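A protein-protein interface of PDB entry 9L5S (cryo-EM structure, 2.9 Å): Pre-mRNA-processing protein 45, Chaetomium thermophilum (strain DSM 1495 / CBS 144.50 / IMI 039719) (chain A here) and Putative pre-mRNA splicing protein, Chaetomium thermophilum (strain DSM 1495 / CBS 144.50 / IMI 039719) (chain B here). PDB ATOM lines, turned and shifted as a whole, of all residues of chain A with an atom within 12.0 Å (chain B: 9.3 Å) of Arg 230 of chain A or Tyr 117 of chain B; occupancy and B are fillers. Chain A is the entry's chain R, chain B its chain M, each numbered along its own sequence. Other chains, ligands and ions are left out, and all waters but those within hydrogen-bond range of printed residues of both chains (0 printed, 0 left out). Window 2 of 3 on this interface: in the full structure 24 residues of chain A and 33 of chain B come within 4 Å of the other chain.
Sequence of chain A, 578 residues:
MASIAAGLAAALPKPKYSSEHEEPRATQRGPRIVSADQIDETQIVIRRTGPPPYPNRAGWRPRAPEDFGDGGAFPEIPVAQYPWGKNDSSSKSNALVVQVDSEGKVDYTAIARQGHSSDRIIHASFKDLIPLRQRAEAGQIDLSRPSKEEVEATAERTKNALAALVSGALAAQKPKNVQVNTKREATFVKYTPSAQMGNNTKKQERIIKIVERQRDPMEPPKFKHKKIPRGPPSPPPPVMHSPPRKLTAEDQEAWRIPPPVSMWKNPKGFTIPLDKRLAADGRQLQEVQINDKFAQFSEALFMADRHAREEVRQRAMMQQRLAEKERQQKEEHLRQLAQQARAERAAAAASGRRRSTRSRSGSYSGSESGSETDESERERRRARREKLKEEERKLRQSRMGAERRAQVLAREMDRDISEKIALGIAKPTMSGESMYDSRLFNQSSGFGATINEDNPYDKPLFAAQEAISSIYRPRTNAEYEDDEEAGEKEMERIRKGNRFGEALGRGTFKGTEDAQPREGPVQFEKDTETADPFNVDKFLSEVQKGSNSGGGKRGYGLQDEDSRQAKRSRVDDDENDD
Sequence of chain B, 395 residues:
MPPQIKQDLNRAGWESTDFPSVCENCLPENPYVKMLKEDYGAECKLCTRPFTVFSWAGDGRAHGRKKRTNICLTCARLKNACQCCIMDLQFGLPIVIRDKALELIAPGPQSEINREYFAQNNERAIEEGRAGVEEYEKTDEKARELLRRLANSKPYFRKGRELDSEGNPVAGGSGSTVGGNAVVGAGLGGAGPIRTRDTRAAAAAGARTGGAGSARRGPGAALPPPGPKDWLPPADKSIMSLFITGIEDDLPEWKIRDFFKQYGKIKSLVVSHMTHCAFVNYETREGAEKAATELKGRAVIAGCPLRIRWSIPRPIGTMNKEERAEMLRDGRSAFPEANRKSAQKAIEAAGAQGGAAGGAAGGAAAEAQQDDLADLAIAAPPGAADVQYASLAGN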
ATOM      1  N   LYS A 226      13.834  18.978   9.968  1.00  0.00           N
ATOM      2  CA  LYS A 226      15.044  18.809  10.758  1.00  0.00           C
ATOM      3  C   LYS A 226      15.307  17.328  10.992  1.00  0.00           C
ATOM      4  O   LYS A 226      14.396  16.582  11.368  1.00  0.00           O
ATOM      5  CB  LYS A 226      14.924  19.545  12.093  1.00  0.00           C
ATOM      6  CG  LYS A 226      14.709  21.042  11.947  1.00  0.00           C
ATOM      7  CD  LYS A 226      14.776  21.758  13.287  1.00  0.00           C
ATOM      8  CE  LYS A 226      13.887  21.088  14.323  1.00  0.00           C
ATOM      9  NZ  LYS A 226      12.548  21.733  14.406  1.00  0.00           N
ATOM     10  N   LYS A 227      16.549  16.908  10.768  1.00  0.00           N
ATOM     11  CA  LYS A 227      16.945  15.515  10.958  1.00  0.00           C
ATOM     12  C   LYS A 227      17.462  15.359  12.382  1.00  0.00           C
ATOM     13  O   LYS A 227      18.639  15.599  12.662  1.00  0.00           O
ATOM     14  CB  LYS A 227      17.991  15.103   9.929  1.00  0.00           C
ATOM     15  CG  LYS A 227      18.338  13.626   9.966  1.00  0.00           C
ATOM     16  CD  LYS A 227      19.634  13.343   9.228  1.00  0.00           C
ATOM     17  CE  LYS A 227      19.385  12.541   7.964  1.00  0.00           C
ATOM     18  NZ  LYS A 227      20.652  11.987   7.415  1.00  0.00           N
ATOM     19  N   ILE A 228      16.574  14.956  13.285  1.00  0.00           N
ATOM     20  CA  ILE A 228      16.907  14.745  14.691  1.00  0.00           C
ATOM     21  C   ILE A 228      17.284  13.277  14.856  1.00  0.00           C
ATOM     22  O   ILE A 228      16.614  12.406  14.280  1.00  0.00           O
ATOM     23  CB  ILE A 228      15.730  15.151  15.596  1.00  0.00           C
ATOM     24  CG1 ILE A 228      15.440  16.646  15.446  1.00  0.00           C
ATOM     25  CG2 ILE A 228      15.997  14.814  17.057  1.00  0.00           C
ATOM     26  CD1 ILE A 228      16.652  17.533  15.645  1.00  0.00           C
ATOM     27  N   PRO A 229      18.347  12.955  15.593  1.00  0.00           N
ATOM     28  CA  PRO A 229      18.716  11.549  15.786  1.00  0.00           C
ATOM     29  C   PRO A 229      17.671  10.787  16.587  1.00  0.00           C
ATOM     30  O   PRO A 229      16.827  11.363  17.277  1.00  0.00           O
ATOM     31  CB  PRO A 229      20.043  11.630  16.548  1.00  0.00           C
ATOM     32  CG  PRO A 229      20.582  12.976  16.214  1.00  0.00           C
ATOM     33  CD  PRO A 229      19.378  13.863  16.123  1.00  0.00           C
ATOM     34  N   ARG A 230      17.734   9.464  16.462  1.00  0.00           N
ATOM     35  CA  ARG A 230      16.749   8.591  17.083  1.00  0.00           C
ATOM     36  C   ARG A 230      16.850   8.641  18.603  1.00  0.00           C
ATOM     37  O   ARG A 230      17.943   8.702  19.170  1.00  0.00           O
ATOM     38  CB  ARG A 230      16.941   7.153  16.602  1.00  0.00           C
ATOM     39  CG  ARG A 230      16.618   6.933  15.136  1.00  0.00           C
ATOM     40  CD  ARG A 230      15.121   6.998  14.890  1.00  0.00           C
ATOM     41  NE  ARG A 230      14.411   5.951  15.615  1.00  0.00           N
ATOM     42  CZ  ARG A 230      13.975   4.824  15.070  1.00  0.00           C
ATOM     43  NH1 ARG A 230      14.163   4.560  13.787  1.00  0.00           N
ATOM     44  NH2 ARG A 230      13.339   3.939  15.830  1.00  0.00           N
ATOM     45  N   GLY A 231      15.694   8.614  19.259  1.00  0.00           N
ATOM     46  CA  GLY A 231      15.638   8.523  20.696  1.00  0.00           C
ATOM     47  C   GLY A 231      16.017   7.136  21.166  1.00  0.00           C
ATOM     48  O   GLY A 231      16.136   6.200  20.368  1.00  0.00           O
ATOM     49  N   PRO A 232      16.239   6.979  22.474  1.00  0.00           N
ATOM     50  CA  PRO A 232      16.560   5.656  23.001  1.00  0.00           C
ATOM     51  C   PRO A 232      15.370   4.725  22.871  1.00  0.00           C
ATOM     52  O   PRO A 232      14.210   5.172  22.873  1.00  0.00           O
ATOM     53  CB  PRO A 232      16.895   5.937  24.476  1.00  0.00           C
ATOM     54  CG  PRO A 232      16.146   7.180  24.791  1.00  0.00           C
ATOM     55  CD  PRO A 232      16.194   7.998  23.535  1.00  0.00           C
ATOM     56  N   PRO A 233      15.605   3.422  22.741  1.00  0.00           N
ATOM     57  CA  PRO A 233      14.490   2.477  22.617  1.00  0.00           C
ATOM     58  C   PRO A 233      13.745   2.317  23.933  1.00  0.00           C
ATOM     59  O   PRO A 233      14.095   2.897  24.964  1.00  0.00           O
ATOM     60  CB  PRO A 233      15.176   1.172  22.204  1.00  0.00           C
ATOM     61  CG  PRO A 233      16.574   1.314  22.706  1.00  0.00           C
ATOM     62  CD  PRO A 233      16.906   2.764  22.538  1.00  0.00           C
ATOM     63  N   SER A 234      12.682   1.519  23.874  1.00  0.00           N
ATOM     64  CA  SER A 234      11.970   1.123  25.076  1.00  0.00           C
ATOM     65  C   SER A 234      12.906   0.325  25.984  1.00  0.00           C
ATOM     66  O   SER A 234      13.846  -0.312  25.498  1.00  0.00           O
ATOM     67  CB  SER A 234      10.737   0.298  24.707  1.00  0.00           C
ATOM     68  OG  SER A 234      11.033  -0.651  23.698  1.00  0.00           O
ATOM     69  N   CYS B  47      11.855  26.097  21.620  1.00  0.00           N
ATOM     70  CA  CYS B  47      12.369  24.861  21.040  1.00  0.00           C
ATOM     71  C   CYS B  47      12.391  24.863  19.518  1.00  0.00           C
ATOM     72  O   CYS B  47      12.860  23.882  18.929  1.00  0.00           O
ATOM     73  CB  CYS B  47      11.550  23.661  21.530  1.00  0.00           C
ATOM     74  SG  CYS B  47       9.793  23.722  21.130  1.00  0.00           S
ATOM     75  N   ARG B  49      10.132  24.374  17.361  1.00  0.00           N
ATOM     76  CA  ARG B  49       9.309  23.384  16.680  1.00  0.00           C
ATOM     77  C   ARG B  49       7.999  24.013  16.222  1.00  0.00           C
ATOM     78  O   ARG B  49       7.476  24.907  16.898  1.00  0.00           O
ATOM     79  CB  ARG B  49       9.007  22.198  17.597  1.00  0.00           C
ATOM     80  CG  ARG B  49       9.996  21.050  17.479  1.00  0.00           C
ATOM     81  CD  ARG B  49      10.100  20.277  18.784  1.00  0.00           C
ATOM     82  NE  ARG B  49       8.997  19.337  18.949  1.00  0.00           N
ATOM     83  CZ  ARG B  49       8.158  19.333  19.976  1.00  0.00           C
ATOM     84  NH1 ARG B  49       8.246  20.229  20.945  1.00  0.00           N
ATOM     85  NH2 ARG B  49       7.203  18.409  20.030  1.00  0.00           N
ATOM     86  N   GLY B 108      14.939  20.998  31.635  1.00  0.00           N
ATOM     87  CA  GLY B 108      15.096  20.758  30.223  1.00  0.00           C
ATOM     88  C   GLY B 108      16.330  21.440  29.673  1.00  0.00           C
ATOM     89  O   GLY B 108      16.726  22.519  30.126  1.00  0.00           O
ATOM     90  N   PRO B 109      16.974  20.809  28.693  1.00  0.00           N
ATOM     91  CA  PRO B 109      18.153  21.420  28.073  1.00  0.00           C
ATOM     92  C   PRO B 109      17.790  22.661  27.276  1.00  0.00           C
ATOM     93  O   PRO B 109      16.676  22.797  26.765  1.00  0.00           O
ATOM     94  CB  PRO B 109      18.689  20.310  27.161  1.00  0.00           C
ATOM     95  CG  PRO B 109      17.502  19.458  26.879  1.00  0.00           C
ATOM     96  CD  PRO B 109      16.693  19.473  28.142  1.00  0.00           C
ATOM     97  N   SER B 111      20.172  23.806  24.885  1.00  0.00           N
ATOM     98  CA  SER B 111      21.071  23.772  23.742  1.00  0.00           C
ATOM     99  C   SER B 111      20.253  23.660  22.455  1.00  0.00           C
ATOM    100  O   SER B 111      19.023  23.752  22.465  1.00  0.00           O
ATOM    101  CB  SER B 111      22.068  22.624  23.888  1.00  0.00           C
ATOM    102  OG  SER B 111      22.886  22.511  22.735  1.00  0.00           O
ATOM    103  N   GLU B 112      20.928  23.452  21.324  1.00  0.00           N
ATOM    104  CA  GLU B 112      20.225  23.465  20.042  1.00  0.00           C
ATOM    105  C   GLU B 112      19.537  22.131  19.765  1.00  0.00           C
ATOM    106  O   GLU B 112      18.308  22.056  19.715  1.00  0.00           O
ATOM    107  CB  GLU B 112      21.201  23.820  18.915  1.00  0.00           C
ATOM    108  CG  GLU B 112      20.591  23.758  17.524  1.00  0.00           C
ATOM    109  CD  GLU B 112      21.632  23.551  16.442  1.00  0.00           C
ATOM    110  OE1 GLU B 112      22.836  23.517  16.774  1.00  0.00           O
ATOM    111  OE2 GLU B 112      21.247  23.422  15.261  1.00  0.00           O
ATOM    112  N   ILE B 113      20.319  21.059  19.624  1.00  0.00           N
ATOM    113  CA  ILE B 113      19.765  19.766  19.227  1.00  0.00           C
ATOM    114  C   ILE B 113      19.130  19.050  20.419  1.00  0.00           C
ATOM    115  O   ILE B 113      18.113  18.348  20.268  1.00  0.00           O
ATOM    116  CB  ILE B 113      20.876  18.933  18.556  1.00  0.00           C
ATOM    117  CG1 ILE B 113      21.217  19.528  17.187  1.00  0.00           C
ATOM    118  CG2 ILE B 113      20.485  17.468  18.396  1.00  0.00           C
ATOM    119  CD1 ILE B 113      22.230  18.727  16.397  1.00  0.00           C
ATOM    120  N   ASN B 114      19.681  19.260  21.619  1.00  0.00           N
ATOM    121  CA  ASN B 114      19.171  18.611  22.823  1.00  0.00           C
ATOM    122  C   ASN B 114      17.743  19.031  23.138  1.00  0.00           C
ATOM    123  O   ASN B 114      17.003  18.270  23.769  1.00  0.00           O
ATOM    124  CB  ASN B 114      20.084  18.921  24.009  1.00  0.00           C
ATOM    125  CG  ASN B 114      21.485  18.386  23.821  1.00  0.00           C
ATOM    126  OD1 ASN B 114      21.677  17.266  23.349  1.00  0.00           O
ATOM    127  ND2 ASN B 114      22.477  19.187  24.187  1.00  0.00           N
ATOM    128  N   ARG B 115      17.333  20.221  22.693  1.00  0.00           N
ATOM    129  CA  ARG B 115      15.957  20.662  22.892  1.00  0.00           C
ATOM    130  C   ARG B 115      14.976  19.778  22.131  1.00  0.00           C
ATOM    131  O   ARG B 115      14.001  19.278  22.710  1.00  0.00           O
ATOM    132  CB  ARG B 115      15.815  22.122  22.465  1.00  0.00           C
ATOM    133  CG  ARG B 115      15.870  23.107  23.614  1.00  0.00           C
ATOM    134  CD  ARG B 115      15.358  24.480  23.214  1.00  0.00           C
ATOM    135  NE  ARG B 115      16.390  25.315  22.611  1.00  0.00           N
ATOM    136  CZ  ARG B 115      16.622  25.413  21.308  1.00  0.00           C
ATOM    137  NH1 ARG B 115      15.907  24.738  20.424  1.00  0.00           N
ATOM    138  NH2 ARG B 115      17.595  26.214  20.882  1.00  0.00           N
ATOM    139  N   GLU B 116      15.222  19.561  20.831  1.00  0.00           N
ATOM    140  CA  GLU B 116      14.364  18.657  20.071  1.00  0.00           C
ATOM    141  C   GLU B 116      14.485  17.224  20.560  1.00  0.00           C
ATOM    142  O   GLU B 116      13.497  16.488  20.534  1.00  0.00           O
ATOM    143  CB  GLU B 116      14.659  18.706  18.570  1.00  0.00           C
ATOM    144  CG  GLU B 116      14.229  19.980  17.869  1.00  0.00           C
ATOM    145  CD  GLU B 116      15.329  21.006  17.820  1.00  0.00           C
ATOM    146  OE1 GLU B 116      16.454  20.661  18.224  1.00  0.00           O
ATOM    147  OE2 GLU B 116      15.071  22.149  17.387  1.00  0.00           O
ATOM    148  N   TYR B 117      15.675  16.810  21.007  1.00  0.00           N
ATOM    149  CA  TYR B 117      15.835  15.455  21.539  1.00  0.00           C
ATOM    150  C   TYR B 117      14.975  15.242  22.785  1.00  0.00           C
ATOM    151  O   TYR B 117      14.234  14.254  22.883  1.00  0.00           O
ATOM    152  CB  TYR B 117      17.310  15.192  21.842  1.00  0.00           C
ATOM    153  CG  TYR B 117      17.691  13.729  21.868  1.00  0.00           C
ATOM    154  CD1 TYR B 117      17.757  12.988  20.695  1.00  0.00           C
ATOM    155  CD2 TYR B 117      18.009  13.094  23.062  1.00  0.00           C
ATOM    156  CE1 TYR B 117      18.110  11.652  20.712  1.00  0.00           C
ATOM    157  CE2 TYR B 117      18.370  11.760  23.089  1.00  0.00           C
ATOM    158  CZ  TYR B 117      18.415  11.045  21.912  1.00  0.00           C
ATOM    159  OH  TYR B 117      18.770   9.716  21.936  1.00  0.00           O
ATOM    160  N   PHE B 118      15.035  16.183  23.731  1.00  0.00           N
ATOM    161  CA  PHE B 118      14.258  16.074  24.961  1.00  0.00           C
ATOM    162  C   PHE B 118      12.761  16.189  24.691  1.00  0.00           C
ATOM    163  O   PHE B 118      11.962  15.470  25.302  1.00  0.00           O
ATOM    164  CB  PHE B 118      14.717  17.144  25.954  1.00  0.00           C
ATOM    165  CG  PHE B 118      14.107  17.013  27.321  1.00  0.00           C
ATOM    166  CD1 PHE B 118      14.629  16.117  28.241  1.00  0.00           C
ATOM    167  CD2 PHE B 118      13.029  17.798  27.694  1.00  0.00           C
ATOM    168  CE1 PHE B 118      14.076  15.997  29.503  1.00  0.00           C
ATOM    169  CE2 PHE B 118      12.471  17.682  28.954  1.00  0.00           C
ATOM    170  CZ  PHE B 118      12.997  16.781  29.859  1.00  0.00           C
ATOM    171  N   ALA B 119      12.362  17.082  23.779  1.00  0.00           N
ATOM    172  CA  ALA B 119      10.944  17.220  23.458  1.00  0.00           C
ATOM    173  C   ALA B 119      10.419  15.993  22.720  1.00  0.00           C
ATOM    174  O   ALA B 119       9.262  15.600  22.904  1.00  0.00           O
ATOM    175  CB  ALA B 119      10.714  18.484  22.632  1.00  0.00           C
ATOM    176  N   GLN B 120      11.254  15.379  21.878  1.00  0.00           N
ATOM    177  CA  GLN B 120      10.861  14.172  21.165  1.00  0.00           C
ATOM    178  C   GLN B 120      10.752  12.982  22.106  1.00  0.00           C
ATOM    179  O   GLN B 120       9.913  12.097  21.904  1.00  0.00           O
ATOM    180  CB  GLN B 120      11.871  13.893  20.051  1.00  0.00           C
ATOM    181  CG  GLN B 120      11.540  12.729  19.140  1.00  0.00           C
ATOM    182  CD  GLN B 120      12.736  12.292  18.316  1.00  0.00           C
ATOM    183  OE1 GLN B 120      13.882  12.571  18.671  1.00  0.00           O
ATOM    184  NE2 GLN B 120      12.476  11.605  17.211  1.00  0.00           N
ATOM    185  N   ASN B 121      11.598  12.932  23.134  1.00  0.00           N
ATOM    186  CA  ASN B 121      11.639  11.772  24.012  1.00  0.00           C
ATOM    187  C   ASN B 121      10.833  11.931  25.297  1.00  0.00           C
ATOM    188  O   ASN B 121      10.714  10.959  26.049  1.00  0.00           O
ATOM    189  CB  ASN B 121      13.090  11.442  24.367  1.00  0.00           C
ATOM    190  CG  ASN B 121      13.920  11.125  23.149  1.00  0.00           C
ATOM    191  OD1 ASN B 121      13.389  10.857  22.073  1.00  0.00           O
ATOM    192  ND2 ASN B 121      15.230  11.172  23.306  1.00  0.00           N
ATOM    193  N   ASN B 122      10.277  13.113  25.573  1.00  0.00           N
ATOM    194  CA  ASN B 122       9.630  13.341  26.859  1.00  0.00           C
ATOM    195  C   ASN B 122       8.256  13.996  26.759  1.00  0.00           C
ATOM    196  O   ASN B 122       7.695  14.366  27.796  1.00  0.00           O
ATOM    197  CB  ASN B 122      10.532  14.192  27.760  1.00  0.00           C
ATOM    198  CG  ASN B 122      11.464  13.352  28.605  1.00  0.00           C
ATOM    199  OD1 ASN B 122      11.077  12.841  29.656  1.00  0.00           O
ATOM    200  ND2 ASN B 122      12.703  13.203  28.151  1.00  0.00           N
ATOM    201  N   GLU B 123       7.687  14.135  25.558  1.00  0.00           N
ATOM    202  CA  GLU B 123       6.451  14.900  25.397  1.00  0.00           C
ATOM    203  C   GLU B 123       5.236  14.228  26.027  1.00  0.00           C
ATOM    204  O   GLU B 123       4.199  14.883  26.169  1.00  0.00           O
ATOM    205  CB  GLU B 123       6.170  15.150  23.910  1.00  0.00           C
ATOM    206  CG  GLU B 123       5.502  13.991  23.161  1.00  0.00           C
ATOM    207  CD  GLU B 123       6.455  12.878  22.740  1.00  0.00           C
ATOM    208  OE1 GLU B 123       7.535  12.719  23.346  1.00  0.00           O
ATOM    209  OE2 GLU B 123       6.114  12.150  21.786  1.00  0.00           O
ATOM    210  N   ILE B 126       5.926  14.993  30.201  1.00  0.00           N
ATOM    211  CA  ILE B 126       5.773  16.408  30.525  1.00  0.00           C
ATOM    212  C   ILE B 126       4.294  16.774  30.609  1.00  0.00           C
ATOM    213  O   ILE B 126       3.885  17.583  31.451  1.00  0.00           O
ATOM    214  CB  ILE B 126       6.531  17.264  29.490  1.00  0.00           C
ATOM    215  CG1 ILE B 126       8.034  17.001  29.586  1.00  0.00           C
ATOM    216  CG2 ILE B 126       6.278  18.748  29.693  1.00  0.00           C
ATOM    217  CD1 ILE B 126       8.814  17.496  28.390  1.00  0.00           C
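NZ of Lys 226 of chain A is in salt-bridge range of OE2 of Glu 116 of chain B. The backbone carbonyl oxygen (O) of Arg 230 of chain A lies within hydrogen-bond range of the side-chain hydroxyl (OH) of Tyr 117 of chain B (3.1 Å). The side-chain amide oxygen (OE1) of Gln 120 of chain B sits close to the backbone carbonyl oxygen (O) of Pro 229 of chain A (3.5 Å).
Of the 9 printed residues of chain A, 6 touch a printed residue of chain B. Hydrophobic or aromatic side chains of chain A that line the printed part of chain B: Ile 228 and Pro 232. Of the 18 printed residues of chain B, 4 touch a printed residue of chain A. Hydrophobic or aromatic side chains of chain B that line the printed part of chain A: Tyr 117. Among the printed residues, Asp or Glu carboxylates within 4 Å of a Lys or Arg side-chain nitrogen of the other chain: Lys 226 of chain A with Glu 116 of chain B (3.9 Å).
Among the printed residues, pairs that only touch across the chains: Ile 228 of chain A with Glu 116 of chain B, Ile 228 of chain A with Gln 120 of chain B, Pro 229 of chain A with Tyr 117 of chain B, Gly 231 of chain A with Tyr 117 of chain B, Gly 231 of chain A with Asn 121 of chain B, Pro 232 of chain A with Tyr 117 of chain B and Pro 232 of chain A with Asn 121 of chain B.
Tyr 117 of chain B touches just these residues of chain A: Pro 229, Arg 230, Gly 231 and Pro 232. Gly 231 of chain A touches just these residues of chain B: Tyr 117 (3.6 Å) and Asn 121 (3.5 Å). No residue of chain A comes within 4 Å of Asn 114 of chain B. Of chain A, only Lys 226 (3.5 Å) and Ile 228 (3.7 Å) come within 4 Å of Glu 116 of chain B. No residue of chain A comes within 4 Å of Phe 118 of chain B. No residue of chain A comes within 4 Å of Ala 119 of chain B. Of chain A, only Ile 228 and Pro 229 come within 4 Å of Gln 120 of chain B. Asn 121 of chain B touches just these residues of chain A: Gly 231 and Pro 232. Printed residues of chain B within 4 Å of Pro 232 of chain A: Tyr 117 (3.5 Å) and Asn 121 (3.3 Å). Printed residues of chain B within 4 Å of Ile 228 of chain A: Glu 116 (3.7 Å) and Gln 120 (3.5 Å). Of the printed residues of chain B, Lys 226 of chain A touches Glu 116 (3.5 Å). Gly 108 of chain B touches none of the printed residues of chain A. The nearest residue of chain B that does not touch Arg 230 of chain A is Gln 120 of chain B (4.9 Å). The nearest residue of chain A that does not touch Tyr 117 of chain B is Ile 228 of chain A (4.4 Å). The nearest printed residue of chain B that does not touch Lys 226 of chain A is Arg 49 of chain B (4.1 Å).
ND2 of Asn 121 of chain B sits close to O of Tyr 117 of chain B (3.3 Å).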
